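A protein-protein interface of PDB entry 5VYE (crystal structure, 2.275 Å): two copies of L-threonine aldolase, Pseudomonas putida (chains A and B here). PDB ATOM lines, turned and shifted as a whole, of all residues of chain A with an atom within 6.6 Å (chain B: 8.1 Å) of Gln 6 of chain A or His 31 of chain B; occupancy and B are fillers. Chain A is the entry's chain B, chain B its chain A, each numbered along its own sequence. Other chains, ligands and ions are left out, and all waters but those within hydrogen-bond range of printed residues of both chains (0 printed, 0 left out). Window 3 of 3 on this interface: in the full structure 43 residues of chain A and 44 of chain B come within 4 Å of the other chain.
Ser 5 of chain A touches just one residue of chain B: His 31. Printed residues of chain A within 4 Å of Asn 28 of chain B: Gly 15. Of chain A, only Ser 5, Gln 6, Tyr 13 and Asp 327 come within 4 Å of His 31 of chain B. Of the printed residues of chain A, Arg 33 of chain B touches Tyr 13 (3.8 Å). Of the printed residues of chain A, Ala 34 of chain B touches Asn 12 (3.96 Å) and Tyr 13 (3.4 Å). The nearest residue of chain B that does not touch Gln 6 of chain A is Gly 30 of chain B (6.0 Å). The nearest residue of chain A that does not touch His 31 of chain B is Ser 14 of chain A (4.03 Å).
Hydrophobic or aromatic side chains of chain B within 4 Å of the printed part of chain A: His 31 and Ala 34. Along chain B the printed residues that touch a printed residue of chain A span positions 28 to 242. Of the 21 printed residues of chain A, 8 touch a printed residue of chain B. Among the printed residues, no Asp or Glu carboxylate lies within 4 Å of a Lys or Arg side-chain nitrogen of the other chain.
No position is printed for both chains.
Gly 30 of chain B touches Lys 4 of chain A. Gln 6 of chain A touches His 31 of chain B (CB to ND1, 3.3 Å). Asn 12 of chain A touches Ala 34 of chain B (O to CB, 3.96 Å). Gly 30 of chain B touches Tyr 13 of chain A. Tyr 13 of chain A touches His 31 of chain B (O to CA, 3.2 Å). Arg 33 of chain B touches Tyr 13 of chain A. Ala 34 of chain B touches Tyr 13 of chain A (N to CE1, 3.4 Å). CA of Gly 15 of chain A touches OD1 of Asn 28 of chain B, at 3.2 Å. Gly 15 of chain A touches Arg 242 of chain B.
The guanidinium group of Arg 242 of chain B sits at hydrogen-bond distance from the backbone carbonyl oxygen of Gly 30 of chain B, 3.4 Å away. O of Gln 6 of chain A sits at hydrogen-bond distance from NH2 of Arg 332 of chain A (2.9 Å). The backbone carbonyl oxygen (O) of Asp 11 of chain A sits at hydrogen-bond distance from the side-chain hydroxyl (OG) of Ser 14 of chain A, at 3.2 Å. The side-chain hydroxyl (OG) of Ser 10 of chain A sits at hydrogen-bond distance from the backbone NH (N) of Asn 12 of chain A. O of Asp 327 of chain A is in hydrogen-bond range of NE2 of Gln 6 of chain A (3.1 Å). The backbone NH (N) of Glu 329 of chain A is in hydrogen-bond range of the side-chain amide oxygen (OE1) of Gln 6 of chain A, at 2.7 Å.
NH2 of Arg 242 of chain B is in hydrogen-bond range of O of Tyr 13 of chain A (3.0 Å). O of Ser 14 of chain A is in hydrogen-bond range of NH2 of Arg 242 of chain B. N of Asp 32 of chain B lies within hydrogen-bond range of O of Tyr 13 of chain A, 3.3 Å away. The side-chain hydroxyl (OG) of Ser 5 of chain A is in hydrogen-bond range of the backbone carbonyl oxygen (O) of His 31 of chain B, 2.5 Å away. A ring nitrogen (NE2) of His 31 of chain B sits close to the side-chain carboxylate (OD1) of Asp 327 of chain A (3.5 Å).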
ATOM      1  N   ASP A   3       8.072  18.821  26.511  1.00  0.00           N
ATOM      2  CA  ASP A   3       6.697  18.415  26.179  1.00  0.00           C
ATOM      3  C   ASP A   3       6.536  17.990  24.686  1.00  0.00           C
ATOM      4  O   ASP A   3       6.982  18.747  23.800  1.00  0.00           O
ATOM      5  CB  ASP A   3       5.688  19.579  26.500  1.00  0.00           C
ATOM      6  CG  ASP A   3       5.298  19.682  28.027  1.00  0.00           C
ATOM      7  OD1 ASP A   3       5.562  18.721  28.787  1.00  0.00           O
ATOM      8  OD2 ASP A   3       4.698  20.714  28.455  1.00  0.00           O
ATOM      9  N   LYS A   4       5.874  16.849  24.375  1.00  0.00           N
ATOM     10  CA  LYS A   4       5.135  15.996  25.337  1.00  0.00           C
ATOM     11  C   LYS A   4       4.634  14.670  24.720  1.00  0.00           C
ATOM     12  O   LYS A   4       4.394  14.564  23.512  1.00  0.00           O
ATOM     13  CB  LYS A   4       3.954  16.795  25.939  1.00  0.00           C
ATOM     14  CG  LYS A   4       3.011  16.072  26.951  1.00  0.00           C
ATOM     15  CD  LYS A   4       3.750  15.640  28.284  1.00  0.00           C
ATOM     16  CE  LYS A   4       2.771  15.205  29.416  1.00  0.00           C
ATOM     17  NZ  LYS A   4       2.607  13.672  29.478  1.00  0.00           N
ATOM     18  N   SER A   5       4.530  13.647  25.580  1.00  0.00           N
ATOM     19  CA  SER A   5       3.996  12.342  25.185  1.00  0.00           C
ATOM     20  C   SER A   5       2.623  12.442  24.521  1.00  0.00           C
ATOM     21  O   SER A   5       2.273  11.588  23.701  1.00  0.00           O
ATOM     22  CB  SER A   5       3.902  11.431  26.415  1.00  0.00           C
ATOM     23  OG  SER A   5       3.887  10.062  26.059  1.00  0.00           O
ATOM     24  N   GLN A   6       1.845  13.477  24.839  1.00  0.00           N
ATOM     25  CA  GLN A   6       0.401  13.467  24.606  1.00  0.00           C
ATOM     26  C   GLN A   6       0.070  14.064  23.238  1.00  0.00           C
ATOM     27  O   GLN A   6       0.399  15.223  22.936  1.00  0.00           O
ATOM     28  CB  GLN A   6      -0.351  14.197  25.721  1.00  0.00           C
ATOM     29  CG  GLN A   6      -0.269  15.737  25.718  1.00  0.00           C
ATOM     30  CD  GLN A   6      -1.288  16.343  26.701  1.00  0.00           C
ATOM     31  OE1 GLN A   6      -2.091  17.223  26.330  1.00  0.00           O
ATOM     32  NE2 GLN A   6      -1.303  15.816  27.947  1.00  0.00           N
ATOM     33  N   GLN A   7      -0.591  13.252  22.420  1.00  0.00           N
ATOM     34  CA  GLN A   7      -0.928  13.568  21.071  1.00  0.00           C
ATOM     35  C   GLN A   7      -2.447  13.703  20.968  1.00  0.00           C
ATOM     36  O   GLN A   7      -3.143  13.808  21.982  1.00  0.00           O
ATOM     37  CB  GLN A   7      -0.355  12.471  20.180  1.00  0.00           C
ATOM     38  CG  GLN A   7       1.186  12.505  20.078  1.00  0.00           C
ATOM     39  CD  GLN A   7       1.689  13.788  19.418  1.00  0.00           C
ATOM     40  OE1 GLN A   7       0.950  14.451  18.677  1.00  0.00           O
ATOM     41  NE2 GLN A   7       2.947  14.158  19.713  1.00  0.00           N
ATOM     42  N   PHE A   8      -2.951  13.685  19.751  1.00  0.00           N
ATOM     43  CA  PHE A   8      -4.362  13.861  19.476  1.00  0.00           C
ATOM     44  C   PHE A   8      -4.870  12.686  18.639  1.00  0.00           C
ATOM     45  O   PHE A   8      -5.786  12.821  17.813  1.00  0.00           O
ATOM     46  CB  PHE A   8      -4.573  15.222  18.822  1.00  0.00           C
ATOM     47  CG  PHE A   8      -4.344  16.374  19.801  1.00  0.00           C
ATOM     48  CD1 PHE A   8      -5.361  16.786  20.639  1.00  0.00           C
ATOM     49  CD2 PHE A   8      -3.091  16.978  19.948  1.00  0.00           C
ATOM     50  CE1 PHE A   8      -5.154  17.806  21.575  1.00  0.00           C
ATOM     51  CE2 PHE A   8      -2.885  17.994  20.874  1.00  0.00           C
ATOM     52  CZ  PHE A   8      -3.919  18.408  21.681  1.00  0.00           C
ATOM     53  N   SER A  10      -5.844   9.338  19.956  1.00  0.00           N
ATOM     54  CA  SER A  10      -6.921   8.553  20.532  1.00  0.00           C
ATOM     55  C   SER A  10      -7.078   8.840  22.014  1.00  0.00           C
ATOM     56  O   SER A  10      -6.081   8.881  22.739  1.00  0.00           O
ATOM     57  CB  SER A  10      -6.640   7.068  20.395  1.00  0.00           C
ATOM     58  OG  SER A  10      -7.698   6.401  21.040  1.00  0.00           O
ATOM     59  N   ASP A  11      -8.346   8.910  22.487  1.00  0.00           N
ATOM     60  CA  ASP A  11      -8.462   8.846  23.954  1.00  0.00           C
ATOM     61  C   ASP A  11      -8.113   7.392  24.547  1.00  0.00           C
ATOM     62  O   ASP A  11      -8.308   7.186  25.772  1.00  0.00           O
ATOM     63  CB  ASP A  11      -9.838   9.350  24.468  1.00  0.00           C
ATOM     64  CG  ASP A  11     -11.066   8.824  23.665  1.00  0.00           C
ATOM     65  OD1 ASP A  11     -10.901   8.242  22.566  1.00  0.00           O
ATOM     66  OD2 ASP A  11     -12.220   9.035  24.152  1.00  0.00           O
ATOM     67  N   ASN A  12      -7.575   6.450  23.763  1.00  0.00           N
ATOM     68  CA  ASN A  12      -7.108   5.160  24.270  1.00  0.00           C
ATOM     69  C   ASN A  12      -5.637   5.172  24.644  1.00  0.00           C
ATOM     70  O   ASN A  12      -5.068   4.109  24.897  1.00  0.00           O
ATOM     71  CB  ASN A  12      -7.312   4.035  23.233  1.00  0.00           C
ATOM     72  CG  ASN A  12      -8.747   3.923  22.734  1.00  0.00           C
ATOM     73  OD1 ASN A  12      -9.601   4.720  23.109  1.00  0.00           O
ATOM     74  ND2 ASN A  12      -9.014   2.951  21.886  1.00  0.00           N
ATOM     75  N   TYR A  13      -4.986   6.320  24.591  1.00  0.00           N
ATOM     76  CA  TYR A  13      -3.584   6.435  24.983  1.00  0.00           C
ATOM     77  C   TYR A  13      -3.428   7.099  26.341  1.00  0.00           C
ATOM     78  O   TYR A  13      -2.319   7.109  26.892  1.00  0.00           O
ATOM     79  CB  TYR A  13      -2.802   7.240  23.925  1.00  0.00           C
ATOM     80  CG  TYR A  13      -2.812   6.641  22.510  1.00  0.00           C
ATOM     81  CD1 TYR A  13      -3.506   5.467  22.223  1.00  0.00           C
ATOM     82  CD2 TYR A  13      -2.109   7.243  21.470  1.00  0.00           C
ATOM     83  CE1 TYR A  13      -3.515   4.913  20.937  1.00  0.00           C
ATOM     84  CE2 TYR A  13      -2.108   6.688  20.178  1.00  0.00           C
ATOM     85  CZ  TYR A  13      -2.818   5.525  19.924  1.00  0.00           C
ATOM     86  OH  TYR A  13      -2.832   4.974  18.664  1.00  0.00           O
ATOM     87  N   SER A  14      -4.520   7.646  26.873  1.00  0.00           N
ATOM     88  CA  SER A  14      -4.558   8.299  28.168  1.00  0.00           C
ATOM     89  C   SER A  14      -4.338   7.288  29.278  1.00  0.00           C
ATOM     90  O   SER A  14      -4.451   6.079  29.093  1.00  0.00           O
ATOM     91  CB  SER A  14      -5.900   9.010  28.379  1.00  0.00           C
ATOM     92  OG  SER A  14      -6.976   8.077  28.572  1.00  0.00           O
ATOM     93  N   GLY A  15      -4.026   7.798  30.455  1.00  0.00           N
ATOM     94  CA  GLY A  15      -3.685   6.954  31.572  1.00  0.00           C
ATOM     95  C   GLY A  15      -4.861   6.680  32.480  1.00  0.00           C
ATOM     96  O   GLY A  15      -6.025   6.956  32.163  1.00  0.00           O
ATOM     97  N   TRP A 309       3.079  16.219  15.472  1.00  0.00           N
ATOM     98  CA  TRP A 309       1.707  16.053  15.891  1.00  0.00           C
ATOM     99  C   TRP A 309       1.239  14.680  15.413  1.00  0.00           C
ATOM    100  O   TRP A 309       1.469  14.303  14.261  1.00  0.00           O
ATOM    101  CB  TRP A 309       0.845  17.167  15.299  1.00  0.00           C
ATOM    102  CG  TRP A 309       1.061  18.485  15.898  1.00  0.00           C
ATOM    103  CD1 TRP A 309       1.278  19.655  15.236  1.00  0.00           C
ATOM    104  CD2 TRP A 309       1.065  18.801  17.295  1.00  0.00           C
ATOM    105  NE1 TRP A 309       1.419  20.679  16.132  1.00  0.00           N
ATOM    106  CE2 TRP A 309       1.296  20.185  17.405  1.00  0.00           C
ATOM    107  CE3 TRP A 309       0.893  18.048  18.463  1.00  0.00           C
ATOM    108  CZ2 TRP A 309       1.352  20.838  18.637  1.00  0.00           C
ATOM    109  CZ3 TRP A 309       0.960  18.691  19.676  1.00  0.00           C
ATOM    110  CH2 TRP A 309       1.187  20.075  19.756  1.00  0.00           C
ATOM    111  N   SER A 325      -8.583  13.802  25.450  1.00  0.00           N
ATOM    112  CA  SER A 325      -8.848  12.897  26.556  1.00  0.00           C
ATOM    113  C   SER A 325      -8.961  13.666  27.869  1.00  0.00           C
ATOM    114  O   SER A 325      -8.839  14.894  27.931  1.00  0.00           O
ATOM    115  CB  SER A 325      -7.741  11.856  26.689  1.00  0.00           C
ATOM    116  OG  SER A 325      -7.484  11.256  25.453  1.00  0.00           O
ATOM    117  N   ASP A 327      -6.983  13.925  30.172  1.00  0.00           N
ATOM    118  CA  ASP A 327      -5.706  14.463  30.625  1.00  0.00           C
ATOM    119  C   ASP A 327      -4.995  15.270  29.548  1.00  0.00           C
ATOM    120  O   ASP A 327      -3.803  15.560  29.684  1.00  0.00           O
ATOM    121  CB  ASP A 327      -4.787  13.330  31.107  1.00  0.00           C
ATOM    122  CG  ASP A 327      -4.522  12.293  30.032  1.00  0.00           C
ATOM    123  OD1 ASP A 327      -5.270  12.247  29.039  1.00  0.00           O
ATOM    124  OD2 ASP A 327      -3.572  11.510  30.199  1.00  0.00           O
ATOM    125  N   THR A 328      -5.686  15.627  28.482  1.00  0.00           N
ATOM    126  CA  THR A 328      -5.161  16.593  27.545  1.00  0.00           C
ATOM    127  C   THR A 328      -4.959  17.959  28.211  1.00  0.00           C
ATOM    128  O   THR A 328      -5.841  18.479  28.906  1.00  0.00           O
ATOM    129  CB  THR A 328      -6.118  16.678  26.355  1.00  0.00           C
ATOM    130  OG1 THR A 328      -6.130  15.403  25.687  1.00  0.00           O
ATOM    131  CG2 THR A 328      -5.682  17.777  25.376  1.00  0.00           C
ATOM    132  N   GLU A 329      -3.778  18.536  28.017  1.00  0.00           N
ATOM    133  CA  GLU A 329      -3.508  19.877  28.522  1.00  0.00           C
ATOM    134  C   GLU A 329      -4.037  20.882  27.523  1.00  0.00           C
ATOM    135  O   GLU A 329      -3.793  20.762  26.313  1.00  0.00           O
ATOM    136  CB  GLU A 329      -2.016  20.072  28.762  1.00  0.00           C
ATOM    137  CG  GLU A 329      -1.458  19.282  29.969  1.00  0.00           C
ATOM    138  CD  GLU A 329       0.005  18.800  29.777  1.00  0.00           C
ATOM    139  OE1 GLU A 329       0.498  18.767  28.622  1.00  0.00           O
ATOM    140  OE2 GLU A 329       0.673  18.441  30.782  1.00  0.00           O
ATOM    141  N   GLU A 330      -4.813  21.846  28.024  1.00  0.00           N
ATOM    142  CA  GLU A 330      -5.263  22.957  27.186  1.00  0.00           C
ATOM    143  C   GLU A 330      -4.092  23.610  26.458  1.00  0.00           C
ATOM    144  O   GLU A 330      -4.222  24.015  25.301  1.00  0.00           O
ATOM    145  CB  GLU A 330      -6.019  23.980  28.035  1.00  0.00           C
ATOM    146  CG  GLU A 330      -6.121  25.368  27.388  1.00  0.00           C
ATOM    147  CD  GLU A 330      -6.433  26.478  28.387  1.00  0.00           C
ATOM    148  OE1 GLU A 330      -6.930  26.149  29.484  1.00  0.00           O
ATOM    149  OE2 GLU A 330      -6.184  27.670  28.058  1.00  0.00           O
ATOM    150  N   GLU A 331      -2.925  23.701  27.096  1.00  0.00           N
ATOM    151  CA  GLU A 331      -1.816  24.362  26.414  1.00  0.00           C
ATOM    152  C   GLU A 331      -1.386  23.593  25.168  1.00  0.00           C
ATOM    153  O   GLU A 331      -1.055  24.208  24.151  1.00  0.00           O
ATOM    154  CB  GLU A 331      -0.634  24.577  27.362  1.00  0.00           C
ATOM    155  CG  GLU A 331       0.531  25.392  26.747  1.00  0.00           C
ATOM    156  CD  GLU A 331       0.117  26.799  26.193  1.00  0.00           C
ATOM    157  OE1 GLU A 331      -0.509  27.599  26.942  1.00  0.00           O
ATOM    158  OE2 GLU A 331       0.426  27.099  25.002  1.00  0.00           O
ATOM    159  N   ARG A 332      -1.375  22.257  25.220  1.00  0.00           N
ATOM    160  CA  ARG A 332      -1.070  21.468  24.019  1.00  0.00           C
ATOM    161  C   ARG A 332      -2.064  21.776  22.910  1.00  0.00           C
ATOM    162  O   ARG A 332      -1.689  21.937  21.741  1.00  0.00           O
ATOM    163  CB  ARG A 332      -1.059  19.966  24.344  1.00  0.00           C
ATOM    164  CG  ARG A 332       0.197  19.456  25.116  1.00  0.00           C
ATOM    165  CD  ARG A 332       1.488  19.392  24.265  1.00  0.00           C
ATOM    166  NE  ARG A 332       1.549  18.205  23.391  1.00  0.00           N
ATOM    167  CZ  ARG A 332       2.481  17.989  22.455  1.00  0.00           C
ATOM    168  NH1 ARG A 332       3.445  18.872  22.247  1.00  0.00           N
ATOM    169  NH2 ARG A 332       2.456  16.883  21.714  1.00  0.00           N
ATOM    170  N   VAL A 333      -3.338  21.911  23.264  1.00  0.00           N
ATOM    171  CA  VAL A 333      -4.335  22.328  22.280  1.00  0.00           C
ATOM    172  C   VAL A 333      -3.961  23.677  21.671  1.00  0.00           C
ATOM    173  O   VAL A 333      -4.016  23.864  20.446  1.00  0.00           O
ATOM    174  CB  VAL A 333      -5.732  22.381  22.926  1.00  0.00           C
ATOM    175  CG1 VAL A 333      -6.762  22.806  21.891  1.00  0.00           C
ATOM    176  CG2 VAL A 333      -6.081  21.051  23.624  1.00  0.00           C
ATOM    177  N   ALA B  27       4.105   2.806  34.718  1.00  0.00           N
ATOM    178  CA  ALA B  27       3.501   2.847  33.383  1.00  0.00           C
ATOM    179  C   ALA B  27       2.413   3.897  33.285  1.00  0.00           C
ATOM    180  O   ALA B  27       2.016   4.251  32.183  1.00  0.00           O
ATOM    181  CB  ALA B  27       2.912   1.499  32.998  1.00  0.00           C
ATOM    182  N   ASN B  28       1.908   4.392  34.403  1.00  0.00           N
ATOM    183  CA  ASN B  28       0.881   5.427  34.348  1.00  0.00           C
ATOM    184  C   ASN B  28       1.463   6.835  34.285  1.00  0.00           C
ATOM    185  O   ASN B  28       0.943   7.718  34.960  1.00  0.00           O
ATOM    186  CB  ASN B  28      -0.075   5.321  35.536  1.00  0.00           C
ATOM    187  CG  ASN B  28      -1.419   6.011  35.253  1.00  0.00           C
ATOM    188  OD1 ASN B  28      -1.857   6.089  34.087  1.00  0.00           O
ATOM    189  ND2 ASN B  28      -2.083   6.504  36.306  1.00  0.00           N
ATOM    190  N   HIS B  29       2.505   7.090  33.492  1.00  0.00           N
ATOM    191  CA  HIS B  29       3.031   8.444  33.309  1.00  0.00           C
ATOM    192  C   HIS B  29       3.230   8.710  31.827  1.00  0.00           C
ATOM    193  O   HIS B  29       4.310   8.469  31.275  1.00  0.00           O
ATOM    194  CB  HIS B  29       4.294   8.638  34.128  1.00  0.00           C
ATOM    195  CG  HIS B  29       4.029   8.468  35.587  1.00  0.00           C
ATOM    196  ND1 HIS B  29       3.122   9.257  36.267  1.00  0.00           N
ATOM    197  CD2 HIS B  29       4.446   7.529  36.467  1.00  0.00           C
ATOM    198  CE1 HIS B  29       3.026   8.834  37.517  1.00  0.00           C
ATOM    199  NE2 HIS B  29       3.822   7.789  37.666  1.00  0.00           N
ATOM    200  N   GLY B  30       2.148   9.219  31.210  1.00  0.00           N
ATOM    201  CA  GLY B  30       2.113   9.840  29.906  1.00  0.00           C
ATOM    202  C   GLY B  30       0.950   9.324  29.073  1.00  0.00           C
ATOM    203  O   GLY B  30      -0.049   8.816  29.598  1.00  0.00           O
ATOM    204  N   HIS B  31       1.076   9.539  27.766  1.00  0.00           N
ATOM    205  CA  HIS B  31       0.326   8.832  26.741  1.00  0.00           C
ATOM    206  C   HIS B  31       1.250   7.786  26.120  1.00  0.00           C
ATOM    207  O   HIS B  31       2.472   7.965  26.083  1.00  0.00           O
ATOM    208  CB  HIS B  31      -0.181   9.793  25.646  1.00  0.00           C
ATOM    209  CG  HIS B  31      -1.344  10.654  26.051  1.00  0.00           C
ATOM    210  ND1 HIS B  31      -1.330  11.448  27.179  1.00  0.00           N
ATOM    211  CD2 HIS B  31      -2.546  10.866  25.458  1.00  0.00           C
ATOM    212  CE1 HIS B  31      -2.478  12.099  27.271  1.00  0.00           C
ATOM    213  NE2 HIS B  31      -3.233  11.765  26.240  1.00  0.00           N
ATOM    214  N   ASP B  32       0.668   6.684  25.639  1.00  0.00           N
ATOM    215  CA  ASP B  32       1.450   5.729  24.861  1.00  0.00           C
ATOM    216  C   ASP B  32       0.521   5.005  23.891  1.00  0.00           C
ATOM    217  O   ASP B  32      -0.672   4.848  24.155  1.00  0.00           O
ATOM    218  CB  ASP B  32       2.215   4.755  25.789  1.00  0.00           C
ATOM    219  CG  ASP B  32       3.567   4.320  25.208  1.00  0.00           C
ATOM    220  OD1 ASP B  32       3.720   4.247  23.956  1.00  0.00           O
ATOM    221  OD2 ASP B  32       4.482   4.045  26.018  1.00  0.00           O
ATOM    222  N   ARG B  33       1.063   4.598  22.745  1.00  0.00           N
ATOM    223  CA  ARG B  33       0.239   3.956  21.729  1.00  0.00           C
ATOM    224  C   ARG B  33      -0.339   2.627  22.237  1.00  0.00           C
ATOM    225  O   ARG B  33       0.264   1.934  23.070  1.00  0.00           O
ATOM    226  CB  ARG B  33       1.056   3.746  20.456  1.00  0.00           C
ATOM    227  CG  ARG B  33       1.339   5.045  19.719  1.00  0.00           C
ATOM    228  CD  ARG B  33       2.123   4.823  18.438  1.00  0.00           C
ATOM    229  NE  ARG B  33       3.424   4.214  18.704  1.00  0.00           N
ATOM    230  CZ  ARG B  33       4.389   4.070  17.798  1.00  0.00           C
ATOM    231  NH1 ARG B  33       4.207   4.496  16.555  1.00  0.00           N
ATOM    232  NH2 ARG B  33       5.538   3.496  18.138  1.00  0.00           N
ATOM    233  N   ALA B  34      -1.521   2.272  21.699  1.00  0.00           N
ATOM    234  CA  ALA B  34      -2.391   1.224  22.232  1.00  0.00           C
ATOM    235  C   ALA B  34      -2.124  -0.120  21.564  1.00  0.00           C
ATOM    236  O   ALA B  34      -1.309  -0.251  20.648  1.00  0.00           O
ATOM    237  CB  ALA B  34      -3.878   1.607  22.063  1.00  0.00           C
ATOM    238  N   ASP B  38       4.137  -0.453  22.197  1.00  0.00           N
ATOM    239  CA  ASP B  38       4.359   0.184  23.484  1.00  0.00           C
ATOM    240  C   ASP B  38       5.714  -0.232  24.057  1.00  0.00           C
ATOM    241  O   ASP B  38       6.202  -1.335  23.784  1.00  0.00           O
ATOM    242  CB  ASP B  38       3.176  -0.184  24.394  1.00  0.00           C
ATOM    243  CG  ASP B  38       3.458   0.043  25.812  1.00  0.00           C
ATOM    244  OD1 ASP B  38       3.570   1.232  26.214  1.00  0.00           O
ATOM    245  OD2 ASP B  38       3.564  -0.980  26.516  1.00  0.00           O
ATOM    246  N   GLN B  39       6.326   0.670  24.855  1.00  0.00           N
ATOM    247  CA  GLN B  39       7.631   0.375  25.444  1.00  0.00           C
ATOM    248  C   GLN B  39       7.534  -0.702  26.532  1.00  0.00           C
ATOM    249  O   GLN B  39       8.439  -1.538  26.664  1.00  0.00           O
ATOM    250  CB  GLN B  39       8.276   1.653  25.999  1.00  0.00           C
ATOM    251  CG  GLN B  39       7.693   2.162  27.334  1.00  0.00           C
ATOM    252  CD  GLN B  39       8.607   3.112  28.138  1.00  0.00           C
ATOM    253  OE1 GLN B  39       8.810   2.911  29.336  1.00  0.00           O
ATOM    254  NE2 GLN B  39       9.136   4.142  27.491  1.00  0.00           N
ATOM    255  N   ARG B 242      -0.149  -1.579  28.159  1.00  0.00           N
ATOM    256  CA  ARG B 242       0.932  -1.382  29.148  1.00  0.00           C
ATOM    257  C   ARG B 242       0.522  -1.856  30.532  1.00  0.00           C
ATOM    258  O   ARG B 242       1.354  -2.346  31.297  1.00  0.00           O
ATOM    259  CB  ARG B 242       1.384   0.109  29.222  1.00  0.00           C
ATOM    260  CG  ARG B 242       0.342   1.088  29.587  1.00  0.00           C
ATOM    261  CD  ARG B 242       0.740   2.628  29.499  1.00  0.00           C
ATOM    262  NE  ARG B 242      -0.486   3.369  29.193  1.00  0.00           N
ATOM    263  CZ  ARG B 242      -0.723   4.648  29.442  1.00  0.00           C
ATOM    264  NH1 ARG B 242       0.191   5.442  30.001  1.00  0.00           N
ATOM    265  NH2 ARG B 242      -1.915   5.127  29.114  1.00  0.00           N
